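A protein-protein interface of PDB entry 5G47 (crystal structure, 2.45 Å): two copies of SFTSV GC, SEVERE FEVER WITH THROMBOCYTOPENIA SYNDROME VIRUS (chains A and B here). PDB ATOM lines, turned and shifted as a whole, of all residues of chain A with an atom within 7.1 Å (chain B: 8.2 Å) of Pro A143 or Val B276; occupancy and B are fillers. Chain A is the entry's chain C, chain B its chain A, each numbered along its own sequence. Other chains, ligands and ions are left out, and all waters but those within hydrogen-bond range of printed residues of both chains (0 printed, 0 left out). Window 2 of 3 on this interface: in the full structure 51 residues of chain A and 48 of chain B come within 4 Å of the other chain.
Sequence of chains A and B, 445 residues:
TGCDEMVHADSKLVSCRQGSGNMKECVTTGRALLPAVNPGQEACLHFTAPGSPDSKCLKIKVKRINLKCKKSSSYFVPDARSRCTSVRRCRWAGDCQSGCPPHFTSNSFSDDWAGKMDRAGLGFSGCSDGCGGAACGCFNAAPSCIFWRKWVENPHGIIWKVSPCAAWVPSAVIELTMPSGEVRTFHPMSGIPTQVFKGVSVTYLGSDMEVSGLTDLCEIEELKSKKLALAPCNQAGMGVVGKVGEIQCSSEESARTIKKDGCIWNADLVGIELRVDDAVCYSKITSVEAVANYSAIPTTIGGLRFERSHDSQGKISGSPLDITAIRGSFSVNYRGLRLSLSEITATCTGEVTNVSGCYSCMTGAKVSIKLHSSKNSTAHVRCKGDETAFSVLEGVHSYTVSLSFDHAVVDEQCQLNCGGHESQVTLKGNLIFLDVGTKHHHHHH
SG of Cys A90 is disulfide-bonded to SG of Cys A138, 2.0 Å away. The backbone NH (N) of Cys A100 lies within hydrogen-bond range of the side-chain sulfur (SG) of Cys A145, at 3.7 Å. The backbone NH of Ala A142 lies within hydrogen-bond range of the side-chain amide oxygen of Asn A140 (2.7 Å). The side-chain sulfur (SG) of Cys A96 forms a disulfide with the side-chain sulfur (SG) of Cys A145, at 2.0 Å. O of Pro A143 sits at hydrogen-bond distance from NH2 of Arg A91, 2.8 Å away. The guanidinium group (NH1) of Arg B275 lies within salt-bridge range of the side-chain carboxylate (OD2) of Asp B278 (3.95 Å).
6 positions are printed for both chains.
Hydrophobic or aromatic side chains of chain B that line the printed part of chain A: Ala B135 and Val B276. Along chain B the printed residues that touch a printed residue of chain A span positions 135 to 276. Of the 20 printed residues of chain A, 6 touch a printed residue of chain B. Printed residues of chain A that touch a printed residue of chain B: Cys A100, Ser A128, Asp A129, Ala A141, Ala A142 and Pro A143. Hydrophobic or aromatic side chains of chain A that line the printed part of chain B: Ala A141, Ala A142 and Pro A143. Among the printed residues, 7 pairs touch across the chains. Among the printed residues, no Asp or Glu carboxylate lies within 4 Å of a Lys or Arg side-chain nitrogen of the other chain.
NH1 of Arg B275 touches CB of Cys A100, at 3.7 Å. Arg B275 touches Asp A129 (CB to OD2, 3.2 Å). O of Ala A141 touches CB of Ala B135, at 3.4 Å. Ala B135 touches Ala A142. Pro A143 touches Val B276.
The side-chain carboxylate of Asp A129 lies within hydrogen-bond range of the backbone NH of Val B276 (2.4 Å). The side-chain carboxylate of Glu B273 is in hydrogen-bond range of the side-chain hydroxyl of Ser A128 (3.2 Å).
Printed residues of chain B within 4 Å of Pro A143: Val B276 (3.98 Å). Ala A142 touches just one residue of chain B: Ala B135. Of the printed residues of chain B, Cys A100 touches Arg B275. Of the printed residues of chain A, Arg B275 touches Cys A100 (3.7 Å) and Asp A129 (3.2 Å). Arg A91 touches none of the printed residues of chain B. Cys A138 touches none of the printed residues of chain B. The nearest printed residue of chain A that does not touch Glu B273 is Asp A129 (6.3 Å).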
ATOM      1  N   ARG A  89     -11.297 -14.396  28.212  1.00  0.00           N
ATOM      2  CA  ARG A  89     -11.702 -15.735  27.809  1.00  0.00           C
ATOM      3  C   ARG A  89     -10.850 -16.187  26.634  1.00  0.00           C
ATOM      4  O   ARG A  89     -10.552 -15.396  25.735  1.00  0.00           O
ATOM      5  CB  ARG A  89     -13.184 -15.780  27.419  1.00  0.00           C
ATOM      6  CG  ARG A  89     -14.136 -15.334  28.514  1.00  0.00           C
ATOM      7  CD  ARG A  89     -14.028 -16.223  29.742  1.00  0.00           C
ATOM      8  NE  ARG A  89     -14.273 -17.628  29.429  1.00  0.00           N
ATOM      9  CZ  ARG A  89     -15.479 -18.181  29.360  1.00  0.00           C
ATOM     10  NH1 ARG A  89     -16.561 -17.445  29.578  1.00  0.00           N
ATOM     11  NH2 ARG A  89     -15.606 -19.468  29.071  1.00  0.00           N
ATOM     12  N   CYS A  90     -10.468 -17.462  26.639  1.00  0.00           N
ATOM     13  CA  CYS A  90      -9.646 -17.999  25.566  1.00  0.00           C
ATOM     14  C   CYS A  90     -10.431 -18.025  24.251  1.00  0.00           C
ATOM     15  O   CYS A  90     -11.651 -17.841  24.216  1.00  0.00           O
ATOM     16  CB  CYS A  90      -9.145 -19.397  25.928  1.00  0.00           C
ATOM     17  SG  CYS A  90      -8.162 -19.472  27.453  1.00  0.00           S
ATOM     18  N   ARG A  91      -9.707 -18.279  23.154  1.00  0.00           N
ATOM     19  CA  ARG A  91     -10.234 -18.115  21.801  1.00  0.00           C
ATOM     20  C   ARG A  91     -11.357 -19.089  21.450  1.00  0.00           C
ATOM     21  O   ARG A  91     -12.047 -18.869  20.449  1.00  0.00           O
ATOM     22  CB  ARG A  91      -9.091 -18.248  20.789  1.00  0.00           C
ATOM     23  CG  ARG A  91      -9.456 -17.836  19.367  1.00  0.00           C
ATOM     24  CD  ARG A  91      -8.240 -17.523  18.517  1.00  0.00           C
ATOM     25  NE  ARG A  91      -7.764 -16.159  18.725  1.00  0.00           N
ATOM     26  CZ  ARG A  91      -8.144 -15.116  17.994  1.00  0.00           C
ATOM     27  NH1 ARG A  91      -9.010 -15.275  17.002  1.00  0.00           N
ATOM     28  NH2 ARG A  91      -7.658 -13.909  18.256  1.00  0.00           N
ATOM     29  N   CYS A  96     -16.062 -15.283  23.096  1.00  0.00           N
ATOM     30  CA  CYS A  96     -14.842 -15.158  22.310  1.00  0.00           C
ATOM     31  C   CYS A  96     -14.649 -16.373  21.412  1.00  0.00           C
ATOM     32  O   CYS A  96     -13.812 -17.236  21.697  1.00  0.00           O
ATOM     33  CB  CYS A  96     -13.636 -14.978  23.237  1.00  0.00           C
ATOM     34  SG  CYS A  96     -12.038 -14.671  22.434  1.00  0.00           S
ATOM     35  N   SER A  98     -13.264 -17.233  17.989  1.00  0.00           N
ATOM     36  CA  SER A  98     -12.405 -16.716  16.923  1.00  0.00           C
ATOM     37  C   SER A  98     -12.358 -15.186  16.950  1.00  0.00           C
ATOM     38  O   SER A  98     -12.755 -14.504  16.004  1.00  0.00           O
ATOM     39  CB  SER A  98     -12.854 -17.231  15.551  1.00  0.00           C
ATOM     40  OG  SER A  98     -14.098 -16.666  15.173  1.00  0.00           O
ATOM     41  N   GLY A  99     -11.860 -14.657  18.061  1.00  0.00           N
ATOM     42  CA  GLY A  99     -11.708 -13.225  18.203  1.00  0.00           C
ATOM     43  C   GLY A  99     -12.911 -12.561  18.842  1.00  0.00           C
ATOM     44  O   GLY A  99     -13.832 -13.200  19.359  1.00  0.00           O
ATOM     45  N   CYS A 100     -12.889 -11.234  18.800  1.00  0.00           N
ATOM     46  CA  CYS A 100     -13.944 -10.434  19.409  1.00  0.00           C
ATOM     47  C   CYS A 100     -15.214 -10.512  18.568  1.00  0.00           C
ATOM     48  O   CYS A 100     -15.155 -10.317  17.349  1.00  0.00           O
ATOM     49  CB  CYS A 100     -13.502  -8.981  19.554  1.00  0.00           C
ATOM     50  SG  CYS A 100     -12.384  -8.660  20.937  1.00  0.00           S
ATOM     51  N   SER A 128     -11.266  -6.459  23.455  1.00  0.00           N
ATOM     52  CA  SER A 128      -9.900  -6.245  23.007  1.00  0.00           C
ATOM     53  C   SER A 128      -9.159  -7.572  23.053  1.00  0.00           C
ATOM     54  O   SER A 128      -9.630  -8.553  23.635  1.00  0.00           O
ATOM     55  CB  SER A 128      -9.188  -5.197  23.866  1.00  0.00           C
ATOM     56  OG  SER A 128     -10.110  -4.238  24.360  1.00  0.00           O
ATOM     57  N   ASP A 129      -7.980  -7.593  22.438  1.00  0.00           N
ATOM     58  CA  ASP A 129      -7.160  -8.795  22.383  1.00  0.00           C
ATOM     59  C   ASP A 129      -6.206  -8.833  23.570  1.00  0.00           C
ATOM     60  O   ASP A 129      -5.543  -7.838  23.876  1.00  0.00           O
ATOM     61  CB  ASP A 129      -6.379  -8.853  21.071  1.00  0.00           C
ATOM     62  CG  ASP A 129      -7.272  -9.104  19.874  1.00  0.00           C
ATOM     63  OD1 ASP A 129      -8.372  -9.664  20.060  1.00  0.00           O
ATOM     64  OD2 ASP A 129      -6.873  -8.747  18.748  1.00  0.00           O
ATOM     65  N   GLY A 130      -6.145  -9.985  24.238  1.00  0.00           N
ATOM     66  CA  GLY A 130      -5.250 -10.196  25.349  1.00  0.00           C
ATOM     67  C   GLY A 130      -4.173 -11.219  25.039  1.00  0.00           C
ATOM     68  O   GLY A 130      -3.931 -11.588  23.888  1.00  0.00           O
ATOM     69  N   CYS A 131      -3.514 -11.676  26.104  1.00  0.00           N
ATOM     70  CA  CYS A 131      -2.481 -12.694  25.966  1.00  0.00           C
ATOM     71  C   CYS A 131      -3.081 -13.978  25.408  1.00  0.00           C
ATOM     72  O   CYS A 131      -4.257 -14.286  25.620  1.00  0.00           O
ATOM     73  CB  CYS A 131      -1.806 -12.955  27.315  1.00  0.00           C
ATOM     74  SG  CYS A 131      -0.532 -14.239  27.292  1.00  0.00           S
ATOM     75  N   GLY A 132      -2.257 -14.729  24.678  1.00  0.00           N
ATOM     76  CA  GLY A 132      -2.757 -15.861  23.922  1.00  0.00           C
ATOM     77  C   GLY A 132      -2.197 -17.216  24.304  1.00  0.00           C
ATOM     78  O   GLY A 132      -2.964 -18.155  24.519  1.00  0.00           O
ATOM     79  N   GLY A 133      -0.875 -17.337  24.390  1.00  0.00           N
ATOM     80  CA  GLY A 133      -0.198 -18.604  24.612  1.00  0.00           C
ATOM     81  C   GLY A 133      -0.562 -19.376  25.867  1.00  0.00           C
ATOM     82  O   GLY A 133      -1.280 -18.852  26.727  1.00  0.00           O
ATOM     83  N   CYS A 138      -4.176 -20.791  28.210  1.00  0.00           N
ATOM     84  CA  CYS A 138      -5.165 -20.969  27.155  1.00  0.00           C
ATOM     85  C   CYS A 138      -4.752 -22.129  26.263  1.00  0.00           C
ATOM     86  O   CYS A 138      -3.579 -22.256  25.900  1.00  0.00           O
ATOM     87  CB  CYS A 138      -5.336 -19.696  26.315  1.00  0.00           C
ATOM     88  SG  CYS A 138      -6.454 -18.454  27.022  1.00  0.00           S
ATOM     89  N   ASN A 140      -5.732 -22.492  23.130  1.00  0.00           N
ATOM     90  CA  ASN A 140      -5.352 -21.840  21.888  1.00  0.00           C
ATOM     91  C   ASN A 140      -4.135 -20.947  22.106  1.00  0.00           C
ATOM     92  O   ASN A 140      -3.915 -20.409  23.195  1.00  0.00           O
ATOM     93  CB  ASN A 140      -6.526 -21.024  21.350  1.00  0.00           C
ATOM     94  CG  ASN A 140      -6.181 -20.255  20.096  1.00  0.00           C
ATOM     95  OD1 ASN A 140      -5.913 -19.058  20.149  1.00  0.00           O
ATOM     96  ND2 ASN A 140      -6.183 -20.940  18.958  1.00  0.00           N
ATOM     97  N   ALA A 141      -3.332 -20.798  21.052  1.00  0.00           N
ATOM     98  CA  ALA A 141      -2.116 -20.000  21.105  1.00  0.00           C
ATOM     99  C   ALA A 141      -2.293 -18.593  20.548  1.00  0.00           C
ATOM    100  O   ALA A 141      -1.437 -17.737  20.791  1.00  0.00           O
ATOM    101  CB  ALA A 141      -0.982 -20.710  20.355  1.00  0.00           C
ATOM    102  N   ALA A 142      -3.367 -18.335  19.805  1.00  0.00           N
ATOM    103  CA  ALA A 142      -3.640 -16.998  19.311  1.00  0.00           C
ATOM    104  C   ALA A 142      -4.216 -16.131  20.427  1.00  0.00           C
ATOM    105  O   ALA A 142      -4.762 -16.645  21.406  1.00  0.00           O
ATOM    106  CB  ALA A 142      -4.604 -17.062  18.129  1.00  0.00           C
ATOM    107  N   PRO A 143      -4.098 -14.804  20.309  1.00  0.00           N
ATOM    108  CA  PRO A 143      -4.568 -13.922  21.384  1.00  0.00           C
ATOM    109  C   PRO A 143      -6.039 -14.134  21.715  1.00  0.00           C
ATOM    110  O   PRO A 143      -6.849 -14.506  20.862  1.00  0.00           O
ATOM    111  CB  PRO A 143      -4.322 -12.518  20.818  1.00  0.00           C
ATOM    112  CG  PRO A 143      -3.198 -12.697  19.866  1.00  0.00           C
ATOM    113  CD  PRO A 143      -3.409 -14.049  19.245  1.00  0.00           C
ATOM    114  N   SER A 144      -6.372 -13.883  22.981  1.00  0.00           N
ATOM    115  CA  SER A 144      -7.697 -14.088  23.540  1.00  0.00           C
ATOM    116  C   SER A 144      -8.496 -12.787  23.490  1.00  0.00           C
ATOM    117  O   SER A 144      -8.087 -11.803  22.868  1.00  0.00           O
ATOM    118  CB  SER A 144      -7.575 -14.624  24.970  1.00  0.00           C
ATOM    119  OG  SER A 144      -6.858 -13.724  25.802  1.00  0.00           O
ATOM    120  N   CYS A 145      -9.651 -12.784  24.151  1.00  0.00           N
ATOM    121  CA  CYS A 145     -10.529 -11.625  24.222  1.00  0.00           C
ATOM    122  C   CYS A 145     -10.609 -11.134  25.659  1.00  0.00           C
ATOM    123  O   CYS A 145     -10.717 -11.935  26.593  1.00  0.00           O
ATOM    124  CB  CYS A 145     -11.942 -11.949  23.727  1.00  0.00           C
ATOM    125  SG  CYS A 145     -12.059 -12.671  22.082  1.00  0.00           S
ATOM    126  N   SER B  86      -6.482   0.011   9.375  1.00  0.00           N
ATOM    127  CA  SER B  86      -5.244  -0.610   9.823  1.00  0.00           C
ATOM    128  C   SER B  86      -4.977  -1.862   9.002  1.00  0.00           C
ATOM    129  O   SER B  86      -5.905  -2.523   8.526  1.00  0.00           O
ATOM    130  CB  SER B  86      -5.298  -0.959  11.314  1.00  0.00           C
ATOM    131  OG  SER B  86      -6.297  -1.931  11.572  1.00  0.00           O
ATOM    132  N   ARG B  88      -1.975  -5.296   9.080  1.00  0.00           N
ATOM    133  CA  ARG B  88      -0.965  -5.993   9.865  1.00  0.00           C
ATOM    134  C   ARG B  88      -0.095  -6.830   8.939  1.00  0.00           C
ATOM    135  O   ARG B  88      -0.613  -7.589   8.112  1.00  0.00           O
ATOM    136  CB  ARG B  88      -1.618  -6.876  10.930  1.00  0.00           C
ATOM    137  CG  ARG B  88      -0.637  -7.659  11.781  1.00  0.00           C
ATOM    138  CD  ARG B  88      -1.349  -8.383  12.909  1.00  0.00           C
ATOM    139  NE  ARG B  88      -0.605  -9.562  13.335  1.00  0.00           N
ATOM    140  CZ  ARG B  88      -0.788 -10.777  12.831  1.00  0.00           C
ATOM    141  NH1 ARG B  88      -1.696 -10.973  11.884  1.00  0.00           N
ATOM    142  NH2 ARG B  88      -0.064 -11.794  13.271  1.00  0.00           N
ATOM    143  N   ASP B 129       3.462  -2.506  17.160  1.00  0.00           N
ATOM    144  CA  ASP B 129       3.794  -3.920  17.122  1.00  0.00           C
ATOM    145  C   ASP B 129       2.558  -4.764  17.411  1.00  0.00           C
ATOM    146  O   ASP B 129       1.649  -4.345  18.132  1.00  0.00           O
ATOM    147  CB  ASP B 129       4.896  -4.228  18.134  1.00  0.00           C
ATOM    148  CG  ASP B 129       5.948  -3.144  18.181  1.00  0.00           C
ATOM    149  OD1 ASP B 129       6.309  -2.626  17.102  1.00  0.00           O
ATOM    150  OD2 ASP B 129       6.393  -2.794  19.291  1.00  0.00           O
ATOM    151  N   GLY B 130       2.528  -5.961  16.828  1.00  0.00           N
ATOM    152  CA  GLY B 130       1.411  -6.865  17.023  1.00  0.00           C
ATOM    153  C   GLY B 130       1.831  -8.287  17.334  1.00  0.00           C
ATOM    154  O   GLY B 130       2.988  -8.536  17.686  1.00  0.00           O
ATOM    155  N   CYS B 131       0.893  -9.226  17.213  1.00  0.00           N
ATOM    156  CA  CYS B 131       1.203 -10.631  17.442  1.00  0.00           C
ATOM    157  C   CYS B 131       2.257 -11.109  16.451  1.00  0.00           C
ATOM    158  O   CYS B 131       2.327 -10.644  15.310  1.00  0.00           O
ATOM    159  CB  CYS B 131      -0.063 -11.481  17.329  1.00  0.00           C
ATOM    160  SG  CYS B 131       0.215 -13.266  17.414  1.00  0.00           S
ATOM    161  N   GLY B 132       3.085 -12.050  16.897  1.00  0.00           N
ATOM    162  CA  GLY B 132       4.254 -12.435  16.133  1.00  0.00           C
ATOM    163  C   GLY B 132       4.268 -13.855  15.607  1.00  0.00           C
ATOM    164  O   GLY B 132       4.434 -14.066  14.404  1.00  0.00           O
ATOM    165  N   GLY B 133       4.094 -14.835  16.492  1.00  0.00           N
ATOM    166  CA  GLY B 133       4.277 -16.229  16.134  1.00  0.00           C
ATOM    167  C   GLY B 133       3.323 -16.776  15.091  1.00  0.00           C
ATOM    168  O   GLY B 133       2.464 -16.054  14.575  1.00  0.00           O
ATOM    169  N   ALA B 135       0.915 -18.615  15.594  1.00  0.00           N
ATOM    170  CA  ALA B 135      -0.445 -18.653  16.118  1.00  0.00           C
ATOM    171  C   ALA B 135      -1.334 -17.589  15.493  1.00  0.00           C
ATOM    172  O   ALA B 135      -2.562 -17.704  15.562  1.00  0.00           O
ATOM    173  CB  ALA B 135      -0.424 -18.484  17.636  1.00  0.00           C
ATOM    174  N   CYS B 136      -0.746 -16.558  14.887  1.00  0.00           N
ATOM    175  CA  CYS B 136      -1.494 -15.499  14.223  1.00  0.00           C
ATOM    176  C   CYS B 136      -1.087 -15.363  12.758  1.00  0.00           C
ATOM    177  O   CYS B 136      -1.220 -14.290  12.167  1.00  0.00           O
ATOM    178  CB  CYS B 136      -1.318 -14.175  14.963  1.00  0.00           C
ATOM    179  SG  CYS B 136       0.382 -13.831  15.471  1.00  0.00           S
ATOM    180  N   GLY B 137      -0.579 -16.443  12.167  1.00  0.00           N
ATOM    181  CA  GLY B 137      -0.323 -16.486  10.740  1.00  0.00           C
ATOM    182  C   GLY B 137       0.929 -15.776  10.266  1.00  0.00           C
ATOM    183  O   GLY B 137       0.888 -15.036   9.278  1.00  0.00           O
ATOM    184  N   SER B 144       4.956  -8.637  14.861  1.00  0.00           N
ATOM    185  CA  SER B 144       4.705  -8.056  13.548  1.00  0.00           C
ATOM    186  C   SER B 144       4.493  -6.545  13.662  1.00  0.00           C
ATOM    187  O   SER B 144       4.752  -5.927  14.697  1.00  0.00           O
ATOM    188  CB  SER B 144       3.511  -8.750  12.899  1.00  0.00           C
ATOM    189  OG  SER B 144       2.332  -8.551  13.661  1.00  0.00           O
ATOM    190  N   ILE B 146       1.752  -3.231  12.856  1.00  0.00           N
ATOM    191  CA  ILE B 146       0.401  -2.750  12.587  1.00  0.00           C
ATOM    192  C   ILE B 146       0.524  -1.331  12.045  1.00  0.00           C
ATOM    193  O   ILE B 146       0.919  -0.413  12.773  1.00  0.00           O
ATOM    194  CB  ILE B 146      -0.484  -2.782  13.842  1.00  0.00           C
ATOM    195  CG1 ILE B 146      -0.638  -4.214  14.365  1.00  0.00           C
ATOM    196  CG2 ILE B 146      -1.842  -2.149  13.552  1.00  0.00           C
ATOM    197  CD1 ILE B 146      -1.907  -4.909  13.916  1.00  0.00           C
ATOM    198  N   GLU B 273      -8.188   1.914  19.035  1.00  0.00           N
ATOM    199  CA  GLU B 273      -7.563   0.853  19.808  1.00  0.00           C
ATOM    200  C   GLU B 273      -7.118  -0.250  18.858  1.00  0.00           C
ATOM    201  O   GLU B 273      -7.919  -0.743  18.057  1.00  0.00           O
ATOM    202  CB  GLU B 273      -8.519   0.288  20.861  1.00  0.00           C
ATOM    203  CG  GLU B 273      -7.871  -0.737  21.780  1.00  0.00           C
ATOM    204  CD  GLU B 273      -8.823  -1.277  22.827  1.00  0.00           C
ATOM    205  OE1 GLU B 273     -10.021  -1.453  22.516  1.00  0.00           O
ATOM    206  OE2 GLU B 273      -8.371  -1.523  23.965  1.00  0.00           O
ATOM    207  N   LEU B 274      -5.849  -0.630  18.950  1.00  0.00           N
ATOM    208  CA  LEU B 274      -5.278  -1.638  18.068  1.00  0.00           C
ATOM    209  C   LEU B 274      -5.486  -3.025  18.663  1.00  0.00           C
ATOM    210  O   LEU B 274      -4.999  -3.318  19.761  1.00  0.00           O
ATOM    211  CB  LEU B 274      -3.792  -1.378  17.836  1.00  0.00           C
ATOM    212  CG  LEU B 274      -3.440  -0.122  17.041  1.00  0.00           C
ATOM    213  CD1 LEU B 274      -1.940  -0.026  16.885  1.00  0.00           C
ATOM    214  CD2 LEU B 274      -4.126  -0.135  15.684  1.00  0.00           C
ATOM    215  N   ARG B 275      -6.218  -3.865  17.941  1.00  0.00           N
ATOM    216  CA  ARG B 275      -6.314  -5.290  18.210  1.00  0.00           C
ATOM    217  C   ARG B 275      -5.766  -6.048  17.006  1.00  0.00           C
ATOM    218  O   ARG B 275      -5.455  -5.463  15.966  1.00  0.00           O
ATOM    219  CB  ARG B 275      -7.763  -5.705  18.507  1.00  0.00           C
ATOM    220  CG  ARG B 275      -8.803  -4.892  17.753  1.00  0.00           C
ATOM    221  CD  ARG B 275     -10.162  -5.576  17.720  1.00  0.00           C
ATOM    222  NE  ARG B 275     -11.029  -5.200  18.833  1.00  0.00           N
ATOM    223  CZ  ARG B 275     -12.354  -5.308  18.805  1.00  0.00           C
ATOM    224  NH1 ARG B 275     -12.956  -5.767  17.717  1.00  0.00           N
ATOM    225  NH2 ARG B 275     -13.079  -4.948  19.855  1.00  0.00           N
ATOM    226  N   VAL B 276      -5.633  -7.364  17.153  1.00  0.00           N
ATOM    227  CA  VAL B 276      -5.138  -8.178  16.051  1.00  0.00           C
ATOM    228  C   VAL B 276      -6.210  -8.273  14.974  1.00  0.00           C
ATOM    229  O   VAL B 276      -7.384  -8.529  15.269  1.00  0.00           O
ATOM    230  CB  VAL B 276      -4.714  -9.568  16.548  1.00  0.00           C
ATOM    231  CG1 VAL B 276      -4.210 -10.420  15.390  1.00  0.00           C
ATOM    232  CG2 VAL B 276      -3.647  -9.442  17.623  1.00  0.00           C
ATOM    233  N   ASP B 277      -5.811  -8.029  13.726  1.00  0.00           N
ATOM    234  CA  ASP B 277      -6.576  -8.173  12.485  1.00  0.00           C
ATOM    235  C   ASP B 277      -7.521  -7.008  12.199  1.00  0.00           C
ATOM    236  O   ASP B 277      -8.133  -6.996  11.119  1.00  0.00           O
ATOM    237  CB  ASP B 277      -7.388  -9.476  12.427  1.00  0.00           C
ATOM    238  CG  ASP B 277      -6.506 -10.707  12.391  1.00  0.00           C
ATOM    239  OD1 ASP B 277      -5.319 -10.575  12.025  1.00  0.00           O
ATOM    240  OD2 ASP B 277      -6.998 -11.806  12.722  1.00  0.00           O
ATOM    241  N   ASP B 278      -7.665  -6.037  13.101  1.00  0.00           N
ATOM    242  CA  ASP B 278      -8.473  -4.852  12.825  1.00  0.00           C
ATOM    243  C   ASP B 278      -8.271  -3.827  13.927  1.00  0.00           C
ATOM    244  O   ASP B 278      -7.583  -4.079  14.916  1.00  0.00           O
ATOM    245  CB  ASP B 278      -9.961  -5.199  12.701  1.00  0.00           C
ATOM    246  CG  ASP B 278     -10.479  -5.974  13.892  1.00  0.00           C
ATOM    247  OD1 ASP B 278      -9.652  -6.399  14.732  1.00  0.00           O
ATOM    248  OD2 ASP B 278     -11.706  -6.171  13.988  1.00  0.00           O
ATOM    249  N   ALA B 279      -8.892  -2.669  13.744  1.00  0.00           N
ATOM    250  CA  ALA B 279      -8.900  -1.615  14.742  1.00  0.00           C
ATOM    251  C   ALA B 279     -10.298  -1.022  14.833  1.00  0.00           C
ATOM    252  O   ALA B 279     -11.033  -0.964  13.842  1.00  0.00           O
ATOM    253  CB  ALA B 279      -7.886  -0.515  14.413  1.00  0.00           C
